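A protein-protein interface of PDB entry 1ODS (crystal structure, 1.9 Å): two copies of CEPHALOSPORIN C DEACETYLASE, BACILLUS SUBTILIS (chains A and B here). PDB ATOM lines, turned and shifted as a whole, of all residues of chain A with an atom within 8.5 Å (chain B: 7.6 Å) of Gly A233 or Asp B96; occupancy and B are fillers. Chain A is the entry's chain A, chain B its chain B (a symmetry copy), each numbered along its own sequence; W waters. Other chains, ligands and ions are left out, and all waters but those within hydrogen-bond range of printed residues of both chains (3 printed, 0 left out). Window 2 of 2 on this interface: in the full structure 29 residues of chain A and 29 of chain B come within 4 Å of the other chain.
No position is printed for both chains.
Of the 8 pairs that touch across the chains among the printed residues, none has its exchanged pair printed and touching as well.
Among the printed residues, pairs that only touch across the chains: Asn A232 with Asp B96 (3.6 Å), Arg A231 with Tyr B95 (3.6 Å), Arg A231 with Ser B94 (3.6 Å) and Asn A232 with Gln B121 (3.7 Å).
Water W3 bridges O of Arg A230 and OD2 of Asp B96.
Water W1 lies within hydrogen-bond range of the side-chain amide oxygen of Asn A232 (2.7 Å) and the backbone NH of Ser B122 (2.9 Å).
Water W2 lies within hydrogen-bond range of OD1 of Asp B96 (2.8 Å), N of Ser A234 (2.9 Å) and N of Gly A233 (3.2 Å).
The guanidinium group (NH1) of Arg A231 sits at hydrogen-bond distance from the backbone carbonyl oxygen (O) of Ser A227 (3.2 Å).
The backbone carbonyl oxygen of Ser B94 sits at hydrogen-bond distance from the side-chain amide nitrogen of Gln B121, at 3.1 Å.
The backbone NH (N) of Gly B97 sits close to the side-chain hydroxyl (OG) of Ser B94 (3.2 Å).
The side-chain amide oxygen (OE1) of Gln B121 sits at hydrogen-bond distance from the side-chain hydroxyl (OG) of Ser B122 (2.8 Å).
The side-chain hydroxyl of Ser B94 lies within hydrogen-bond range of the side-chain carboxylate of Glu B98.
The backbone carbonyl oxygen of Asp B96 sits at hydrogen-bond distance from the indole nitrogen of Trp B72 (2.9 Å).
The backbone carbonyl oxygen (O) of Arg A231 lies within hydrogen-bond range of the backbone NH (N) of Asp B96 (2.9 Å).
The side-chain amide nitrogen (NE2) of Gln B121 sits at hydrogen-bond distance from the backbone carbonyl oxygen (O) of Arg A231, at 3.1 Å.
NH2 of Arg A230 is in hydrogen-bond range of OH of Tyr B95 (3.4 Å).
OD2 of Asp B96 is in hydrogen-bond range of N of Gly A233 (2.9 Å).
Phe A229 touches none of the printed residues of chain B.
Printed residues of chain B within 4 Å of Asn A232: Asp B96 (3.6 Å) and Gln B121 (3.7 Å).
Gly A233 touches one residue of chain B.
Printed residues of chain A within 4 Å of Ser B94: Arg A231.
Of the printed residues of chain A, Tyr B95 touches Arg A230 and Arg A231.
Of chain A, only Arg A231 (2.9 Å), Asn A232 (3.6 Å) and Gly A233 (2.9 Å) come within 4 Å of Asp B96.
Gly B97 touches none of the printed residues of chain A.
Leu B116 touches none of the printed residues of chain A.
The nearest residue of chain B that does not touch Gly A233 is Tyr B95 (6.7 Å).
The nearest residue of chain A that does not touch Asp B96 is Arg A230 (4.7 Å).
The nearest printed residue of chain B that does not touch Arg A231 is Ala B93 (4.7 Å).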
ATOM      1  N   ASN A 226      25.529 -20.077 -21.177  1.00  0.00           N
ATOM      2  CA  ASN A 226      25.368 -20.689 -22.492  1.00  0.00           C
ATOM      3  C   ASN A 226      24.042 -21.478 -22.603  1.00  0.00           C
ATOM      4  O   ASN A 226      23.297 -21.326 -23.580  1.00  0.00           O
ATOM      5  CB  ASN A 226      26.532 -21.629 -22.801  1.00  0.00           C
ATOM      6  CG  ASN A 226      27.897 -20.991 -22.582  1.00  0.00           C
ATOM      7  OD1 ASN A 226      28.207 -20.528 -21.496  1.00  0.00           O
ATOM      8  ND2 ASN A 226      28.718 -20.996 -23.621  1.00  0.00           N
ATOM      9  N   SER A 227      23.728 -22.280 -21.590  1.00  0.00           N
ATOM     10  CA  SER A 227      22.466 -23.068 -21.543  1.00  0.00           C
ATOM     11  C   SER A 227      21.213 -22.186 -21.574  1.00  0.00           C
ATOM     12  O   SER A 227      20.252 -22.491 -22.258  1.00  0.00           O
ATOM     13  CB  SER A 227      22.426 -23.940 -20.282  1.00  0.00           C
ATOM     14  OG  SER A 227      23.436 -24.949 -20.377  1.00  0.00           O
ATOM     15  N   PHE A 228      21.261 -21.083 -20.850  1.00  0.00           N
ATOM     16  CA  PHE A 228      20.182 -20.095 -20.850  1.00  0.00           C
ATOM     17  C   PHE A 228      19.981 -19.477 -22.261  1.00  0.00           C
ATOM     18  O   PHE A 228      18.860 -19.366 -22.748  1.00  0.00           O
ATOM     19  CB  PHE A 228      20.451 -19.066 -19.744  1.00  0.00           C
ATOM     20  CG  PHE A 228      19.468 -17.941 -19.695  1.00  0.00           C
ATOM     21  CD1 PHE A 228      18.243 -18.091 -19.063  1.00  0.00           C
ATOM     22  CD2 PHE A 228      19.782 -16.714 -20.270  1.00  0.00           C
ATOM     23  CE1 PHE A 228      17.345 -17.034 -19.008  1.00  0.00           C
ATOM     24  CE2 PHE A 228      18.887 -15.654 -20.226  1.00  0.00           C
ATOM     25  CZ  PHE A 228      17.663 -15.813 -19.586  1.00  0.00           C
ATOM     26  N   PHE A 229      21.067 -19.117 -22.937  1.00  0.00           N
ATOM     27  CA  PHE A 229      20.956 -18.541 -24.269  1.00  0.00           C
ATOM     28  C   PHE A 229      20.428 -19.569 -25.277  1.00  0.00           C
ATOM     29  O   PHE A 229      19.734 -19.229 -26.223  1.00  0.00           O
ATOM     30  CB  PHE A 229      22.281 -17.929 -24.756  1.00  0.00           C
ATOM     31  CG  PHE A 229      22.782 -16.784 -23.909  1.00  0.00           C
ATOM     32  CD1 PHE A 229      21.898 -15.934 -23.242  1.00  0.00           C
ATOM     33  CD2 PHE A 229      24.150 -16.538 -23.797  1.00  0.00           C
ATOM     34  CE1 PHE A 229      22.375 -14.898 -22.478  1.00  0.00           C
ATOM     35  CE2 PHE A 229      24.619 -15.491 -23.027  1.00  0.00           C
ATOM     36  CZ  PHE A 229      23.737 -14.686 -22.357  1.00  0.00           C
ATOM     37  N   ARG A 230      20.749 -20.832 -25.062  1.00  0.00           N
ATOM     38  CA  ARG A 230      20.165 -21.894 -25.882  1.00  0.00           C
ATOM     39  C   ARG A 230      18.633 -21.934 -25.750  1.00  0.00           C
ATOM     40  O   ARG A 230      17.924 -22.060 -26.755  1.00  0.00           O
ATOM     41  CB  ARG A 230      20.753 -23.245 -25.496  1.00  0.00           C
ATOM     42  CG  ARG A 230      22.124 -23.463 -26.064  1.00  0.00           C
ATOM     43  CD  ARG A 230      22.864 -24.603 -25.435  1.00  0.00           C
ATOM     44  NE  ARG A 230      22.191 -25.888 -25.597  1.00  0.00           N
ATOM     45  CZ  ARG A 230      22.186 -26.605 -26.711  1.00  0.00           C
ATOM     46  NH1 ARG A 230      22.821 -26.172 -27.787  1.00  0.00           N
ATOM     47  NH2 ARG A 230      21.554 -27.767 -26.757  1.00  0.00           N
ATOM     48  N   ARG A 231      18.147 -21.788 -24.520  1.00  0.00           N
ATOM     49  CA  ARG A 231      16.717 -21.866 -24.191  1.00  0.00           C
ATOM     50  C   ARG A 231      15.915 -20.571 -24.374  1.00  0.00           C
ATOM     51  O   ARG A 231      14.686 -20.607 -24.338  1.00  0.00           O
ATOM     52  CB  ARG A 231      16.552 -22.347 -22.742  1.00  0.00           C
ATOM     53  CG  ARG A 231      17.081 -23.756 -22.529  1.00  0.00           C
ATOM     54  CD  ARG A 231      17.320 -24.145 -21.093  1.00  0.00           C
ATOM     55  NE  ARG A 231      17.502 -25.589 -20.999  1.00  0.00           N
ATOM     56  CZ  ARG A 231      18.560 -26.271 -21.447  1.00  0.00           C
ATOM     57  NH1 ARG A 231      19.602 -25.642 -22.011  1.00  0.00           N
ATOM     58  NH2 ARG A 231      18.592 -27.602 -21.324  1.00  0.00           N
ATOM     59  N   ASN A 232      16.621 -19.456 -24.568  1.00  0.00           N
ATOM     60  CA  ASN A 232      16.065 -18.106 -24.653  1.00  0.00           C
ATOM     61  C   ASN A 232      16.899 -17.396 -25.713  1.00  0.00           C
ATOM     62  O   ASN A 232      17.872 -16.682 -25.438  1.00  0.00           O
ATOM     63  CB  ASN A 232      16.138 -17.373 -23.310  1.00  0.00           C
ATOM     64  CG  ASN A 232      15.456 -18.139 -22.193  1.00  0.00           C
ATOM     65  OD1 ASN A 232      14.282 -17.903 -21.908  1.00  0.00           O
ATOM     66  ND2 ASN A 232      16.181 -19.066 -21.562  1.00  0.00           N
ATOM     67  N   GLY A 233      16.515 -17.637 -26.949  1.00  0.00           N
ATOM     68  CA  GLY A 233      17.395 -17.371 -28.065  1.00  0.00           C
ATOM     69  C   GLY A 233      17.371 -15.979 -28.671  1.00  0.00           C
ATOM     70  O   GLY A 233      18.101 -15.733 -29.636  1.00  0.00           O
ATOM     71  N   SER A 234      16.571 -15.054 -28.154  1.00  0.00           N
ATOM     72  CA  SER A 234      16.540 -13.728 -28.790  1.00  0.00           C
ATOM     73  C   SER A 234      17.882 -12.993 -28.590  1.00  0.00           C
ATOM     74  O   SER A 234      18.480 -13.039 -27.519  1.00  0.00           O
ATOM     75  CB  SER A 234      15.327 -12.881 -28.353  1.00  0.00           C
ATOM     76  OG  SER A 234      15.654 -11.927 -27.384  1.00  0.00           O
ATOM     77  N   PRO A 235      18.365 -12.322 -29.634  1.00  0.00           N
ATOM     78  CA  PRO A 235      19.610 -11.545 -29.531  1.00  0.00           C
ATOM     79  C   PRO A 235      19.575 -10.519 -28.412  1.00  0.00           C
ATOM     80  O   PRO A 235      20.579 -10.377 -27.736  1.00  0.00           O
ATOM     81  CB  PRO A 235      19.686 -10.825 -30.861  1.00  0.00           C
ATOM     82  CG  PRO A 235      18.923 -11.661 -31.768  1.00  0.00           C
ATOM     83  CD  PRO A 235      17.781 -12.247 -30.972  1.00  0.00           C
ATOM     84  N   GLU A 236      18.428  -9.864 -28.224  1.00  0.00           N
ATOM     85  CA  GLU A 236      18.248  -8.854 -27.175  1.00  0.00           C
ATOM     86  C   GLU A 236      18.376  -9.451 -25.785  1.00  0.00           C
ATOM     87  O   GLU A 236      18.884  -8.808 -24.875  1.00  0.00           O
ATOM     88  CB  GLU A 236      16.884  -8.160 -27.314  1.00  0.00           C
ATOM     89  CG  GLU A 236      16.833  -7.170 -28.462  1.00  0.00           C
ATOM     90  CD  GLU A 236      16.921  -7.818 -29.841  1.00  0.00           C
ATOM     91  OE1 GLU A 236      16.293  -8.901 -30.086  1.00  0.00           O
ATOM     92  OE2 GLU A 236      17.627  -7.239 -30.700  1.00  0.00           O
ATOM     93  N   THR A 237      17.907 -10.689 -25.622  1.00  0.00           N
ATOM     94  CA  THR A 237      18.047 -11.388 -24.350  1.00  0.00           C
ATOM     95  C   THR A 237      19.514 -11.580 -24.019  1.00  0.00           C
ATOM     96  O   THR A 237      19.904 -11.418 -22.877  1.00  0.00           O
ATOM     97  CB  THR A 237      17.343 -12.759 -24.375  1.00  0.00           C
ATOM     98  OG1 THR A 237      15.924 -12.574 -24.451  1.00  0.00           O
ATOM     99  CG2 THR A 237      17.550 -13.511 -23.060  1.00  0.00           C
ATOM    100  N   GLU A 238      20.330 -11.942 -25.009  1.00  0.00           N
ATOM    101  CA  GLU A 238      21.766 -12.137 -24.741  1.00  0.00           C
ATOM    102  C   GLU A 238      22.440 -10.821 -24.344  1.00  0.00           C
ATOM    103  O   GLU A 238      23.194 -10.780 -23.376  1.00  0.00           O
ATOM    104  CB  GLU A 238      22.491 -12.752 -25.931  1.00  0.00           C
ATOM    105  CG  GLU A 238      23.969 -13.040 -25.670  1.00  0.00           C
ATOM    106  CD  GLU A 238      24.631 -13.851 -26.774  1.00  0.00           C
ATOM    107  OE1 GLU A 238      23.957 -14.238 -27.760  1.00  0.00           O
ATOM    108  OE2 GLU A 238      25.831 -14.145 -26.649  1.00  0.00           O
ATOM    109  N   ARG B  58       0.388 -15.346 -27.365  1.00  0.00           N
ATOM    110  CA  ARG B  58       1.086 -15.537 -26.123  1.00  0.00           C
ATOM    111  C   ARG B  58       0.040 -15.392 -25.025  1.00  0.00           C
ATOM    112  O   ARG B  58      -0.571 -14.341 -24.900  1.00  0.00           O
ATOM    113  CB  ARG B  58       2.165 -14.491 -25.975  1.00  0.00           C
ATOM    114  CG  ARG B  58       3.070 -14.727 -24.822  1.00  0.00           C
ATOM    115  CD  ARG B  58       3.947 -15.952 -24.981  1.00  0.00           C
ATOM    116  NE  ARG B  58       5.085 -15.879 -24.071  1.00  0.00           N
ATOM    117  CZ  ARG B  58       6.054 -16.779 -24.002  1.00  0.00           C
ATOM    118  NH1 ARG B  58       6.037 -17.860 -24.780  1.00  0.00           N
ATOM    119  NH2 ARG B  58       7.040 -16.586 -23.139  1.00  0.00           N
ATOM    120  N   TRP B  72       2.789 -20.369 -25.301  1.00  0.00           N
ATOM    121  CA  TRP B  72       2.155 -20.166 -26.593  1.00  0.00           C
ATOM    122  C   TRP B  72       0.795 -20.841 -26.590  1.00  0.00           C
ATOM    123  O   TRP B  72       0.640 -21.931 -26.048  1.00  0.00           O
ATOM    124  CB  TRP B  72       3.005 -20.698 -27.734  1.00  0.00           C
ATOM    125  CG  TRP B  72       4.381 -20.128 -27.713  1.00  0.00           C
ATOM    126  CD1 TRP B  72       5.509 -20.793 -27.378  1.00  0.00           C
ATOM    127  CD2 TRP B  72       4.783 -18.776 -27.993  1.00  0.00           C
ATOM    128  NE1 TRP B  72       6.595 -19.959 -27.446  1.00  0.00           N
ATOM    129  CE2 TRP B  72       6.180 -18.712 -27.829  1.00  0.00           C
ATOM    130  CE3 TRP B  72       4.108 -17.612 -28.376  1.00  0.00           C
ATOM    131  CZ2 TRP B  72       6.917 -17.533 -28.027  1.00  0.00           C
ATOM    132  CZ3 TRP B  72       4.840 -16.436 -28.567  1.00  0.00           C
ATOM    133  CH2 TRP B  72       6.225 -16.407 -28.400  1.00  0.00           C
ATOM    134  N   ALA B  93      13.749 -28.383 -20.195  1.00  0.00           N
ATOM    135  CA  ALA B  93      13.828 -28.839 -21.577  1.00  0.00           C
ATOM    136  C   ALA B  93      13.004 -28.027 -22.578  1.00  0.00           C
ATOM    137  O   ALA B  93      12.795 -28.494 -23.692  1.00  0.00           O
ATOM    138  CB  ALA B  93      13.434 -30.304 -21.670  1.00  0.00           C
ATOM    139  N   SER B  94      12.524 -26.838 -22.191  1.00  0.00           N
ATOM    140  CA  SER B  94      11.821 -25.952 -23.117  1.00  0.00           C
ATOM    141  C   SER B  94      12.778 -24.925 -23.699  1.00  0.00           C
ATOM    142  O   SER B  94      13.496 -24.218 -22.960  1.00  0.00           O
ATOM    143  CB  SER B  94      10.664 -25.211 -22.434  1.00  0.00           C
ATOM    144  OG  SER B  94       9.934 -24.445 -23.377  1.00  0.00           O
ATOM    145  N   TYR B  95      12.777 -24.871 -25.029  1.00  0.00           N
ATOM    146  CA  TYR B  95      13.554 -23.963 -25.816  1.00  0.00           C
ATOM    147  C   TYR B  95      12.592 -22.993 -26.460  1.00  0.00           C
ATOM    148  O   TYR B  95      11.878 -23.335 -27.423  1.00  0.00           O
ATOM    149  CB  TYR B  95      14.297 -24.732 -26.905  1.00  0.00           C
ATOM    150  CG  TYR B  95      15.444 -25.539 -26.341  1.00  0.00           C
ATOM    151  CD1 TYR B  95      15.227 -26.669 -25.552  1.00  0.00           C
ATOM    152  CD2 TYR B  95      16.730 -25.172 -26.598  1.00  0.00           C
ATOM    153  CE1 TYR B  95      16.316 -27.395 -25.035  1.00  0.00           C
ATOM    154  CE2 TYR B  95      17.786 -25.873 -26.117  1.00  0.00           C
ATOM    155  CZ  TYR B  95      17.591 -26.957 -25.322  1.00  0.00           C
ATOM    156  OH  TYR B  95      18.737 -27.596 -24.910  1.00  0.00           O
ATOM    157  N   ASP B  96      12.553 -21.793 -25.906  1.00  0.00           N
ATOM    158  CA  ASP B  96      11.620 -20.757 -26.366  1.00  0.00           C
ATOM    159  C   ASP B  96      10.166 -21.252 -26.485  1.00  0.00           C
ATOM    160  O   ASP B  96       9.387 -20.782 -27.327  1.00  0.00           O
ATOM    161  CB  ASP B  96      12.133 -20.125 -27.661  1.00  0.00           C
ATOM    162  CG  ASP B  96      13.247 -19.157 -27.393  1.00  0.00           C
ATOM    163  OD1 ASP B  96      13.039 -18.237 -26.551  1.00  0.00           O
ATOM    164  OD2 ASP B  96      14.368 -19.250 -27.919  1.00  0.00           O
ATOM    165  N   GLY B  97       9.807 -22.179 -25.597  1.00  0.00           N
ATOM    166  CA  GLY B  97       8.424 -22.612 -25.434  1.00  0.00           C
ATOM    167  C   GLY B  97       7.799 -23.517 -26.479  1.00  0.00           C
ATOM    168  O   GLY B  97       6.571 -23.650 -26.493  1.00  0.00           O
ATOM    169  N   GLU B  98       8.612 -24.120 -27.349  1.00  0.00           N
ATOM    170  CA  GLU B  98       8.118 -25.060 -28.349  1.00  0.00           C
ATOM    171  C   GLU B  98       7.004 -24.477 -29.220  1.00  0.00           C
ATOM    172  O   GLU B  98       6.006 -25.162 -29.511  1.00  0.00           O
ATOM    173  CB  GLU B  98       7.612 -26.329 -27.662  1.00  0.00           C
ATOM    174  CG  GLU B  98       8.716 -27.197 -27.070  1.00  0.00           C
ATOM    175  CD  GLU B  98       9.533 -26.467 -26.034  1.00  0.00           C
ATOM    176  OE1 GLU B  98       8.945 -26.062 -24.984  1.00  0.00           O
ATOM    177  OE2 GLU B  98      10.758 -26.260 -26.289  1.00  0.00           O
ATOM    178  N   ILE B  99       7.159 -23.217 -29.629  1.00  0.00           N
ATOM    179  CA  ILE B  99       6.130 -22.574 -30.437  1.00  0.00           C
ATOM    180  C   ILE B  99       5.735 -23.377 -31.686  1.00  0.00           C
ATOM    181  O   ILE B  99       4.570 -23.418 -32.051  1.00  0.00           O
ATOM    182  CB  ILE B  99       6.520 -21.126 -30.805  1.00  0.00           C
ATOM    183  CG1 ILE B  99       5.320 -20.402 -31.445  1.00  0.00           C
ATOM    184  CG2 ILE B  99       7.775 -21.098 -31.693  1.00  0.00           C
ATOM    185  CD1 ILE B  99       5.538 -18.945 -31.693  1.00  0.00           C
ATOM    186  N   HIS B 100       6.703 -24.007 -32.339  1.00  0.00           N
ATOM    187  CA  HIS B 100       6.437 -24.737 -33.576  1.00  0.00           C
ATOM    188  C   HIS B 100       5.588 -25.962 -33.349  1.00  0.00           C
ATOM    189  O   HIS B 100       4.714 -26.275 -34.143  1.00  0.00           O
ATOM    190  CB  HIS B 100       7.747 -25.096 -34.249  1.00  0.00           C
ATOM    191  CG  HIS B 100       8.630 -23.910 -34.447  1.00  0.00           C
ATOM    192  ND1 HIS B 100       8.221 -22.800 -35.161  1.00  0.00           N
ATOM    193  CD2 HIS B 100       9.858 -23.615 -33.957  1.00  0.00           C
ATOM    194  CE1 HIS B 100       9.184 -21.898 -35.148  1.00  0.00           C
ATOM    195  NE2 HIS B 100      10.185 -22.365 -34.421  1.00  0.00           N
ATOM    196  N   LEU B 116       4.257 -23.099 -19.799  1.00  0.00           N
ATOM    197  CA  LEU B 116       5.680 -23.065 -19.477  1.00  0.00           C
ATOM    198  C   LEU B 116       5.908 -23.036 -17.969  1.00  0.00           C
ATOM    199  O   LEU B 116       5.235 -22.324 -17.224  1.00  0.00           O
ATOM    200  CB  LEU B 116       6.391 -21.935 -20.198  1.00  0.00           C
ATOM    201  CG  LEU B 116       6.146 -21.981 -21.706  1.00  0.00           C
ATOM    202  CD1 LEU B 116       6.806 -20.774 -22.405  1.00  0.00           C
ATOM    203  CD2 LEU B 116       6.593 -23.309 -22.351  1.00  0.00           C
ATOM    204  N   GLN B 121      11.231 -21.806 -17.651  1.00  0.00           N
ATOM    205  CA  GLN B 121      11.087 -21.211 -18.975  1.00  0.00           C
ATOM    206  C   GLN B 121       9.962 -20.173 -18.947  1.00  0.00           C
ATOM    207  O   GLN B 121       8.805 -20.519 -18.691  1.00  0.00           O
ATOM    208  CB  GLN B 121      10.812 -22.292 -20.022  1.00  0.00           C
ATOM    209  CG  GLN B 121      10.405 -21.756 -21.388  1.00  0.00           C
ATOM    210  CD  GLN B 121      11.456 -20.873 -22.011  1.00  0.00           C
ATOM    211  OE1 GLN B 121      11.158 -19.766 -22.433  1.00  0.00           O
ATOM    212  NE2 GLN B 121      12.680 -21.367 -22.087  1.00  0.00           N
ATOM    213  N   SER B 122      10.335 -18.905 -19.148  1.00  0.00           N
ATOM    214  CA  SER B 122       9.412 -17.770 -19.298  1.00  0.00           C
ATOM    215  C   SER B 122       8.530 -17.457 -18.078  1.00  0.00           C
ATOM    216  O   SER B 122       8.413 -16.302 -17.677  1.00  0.00           O
ATOM    217  CB  SER B 122       8.543 -17.966 -20.543  1.00  0.00           C
ATOM    218  OG  SER B 122       9.313 -17.794 -21.711  1.00  0.00           O
HETATM  219  O   HOH W   1      13.106 -18.301 -19.464  1.00  0.00           O
HETATM  220  O   HOH W   2      14.082 -15.639 -26.732  1.00  0.00           O
HETATM  221  O   HOH W   3      15.842 -21.700 -28.422  1.00  0.00           O
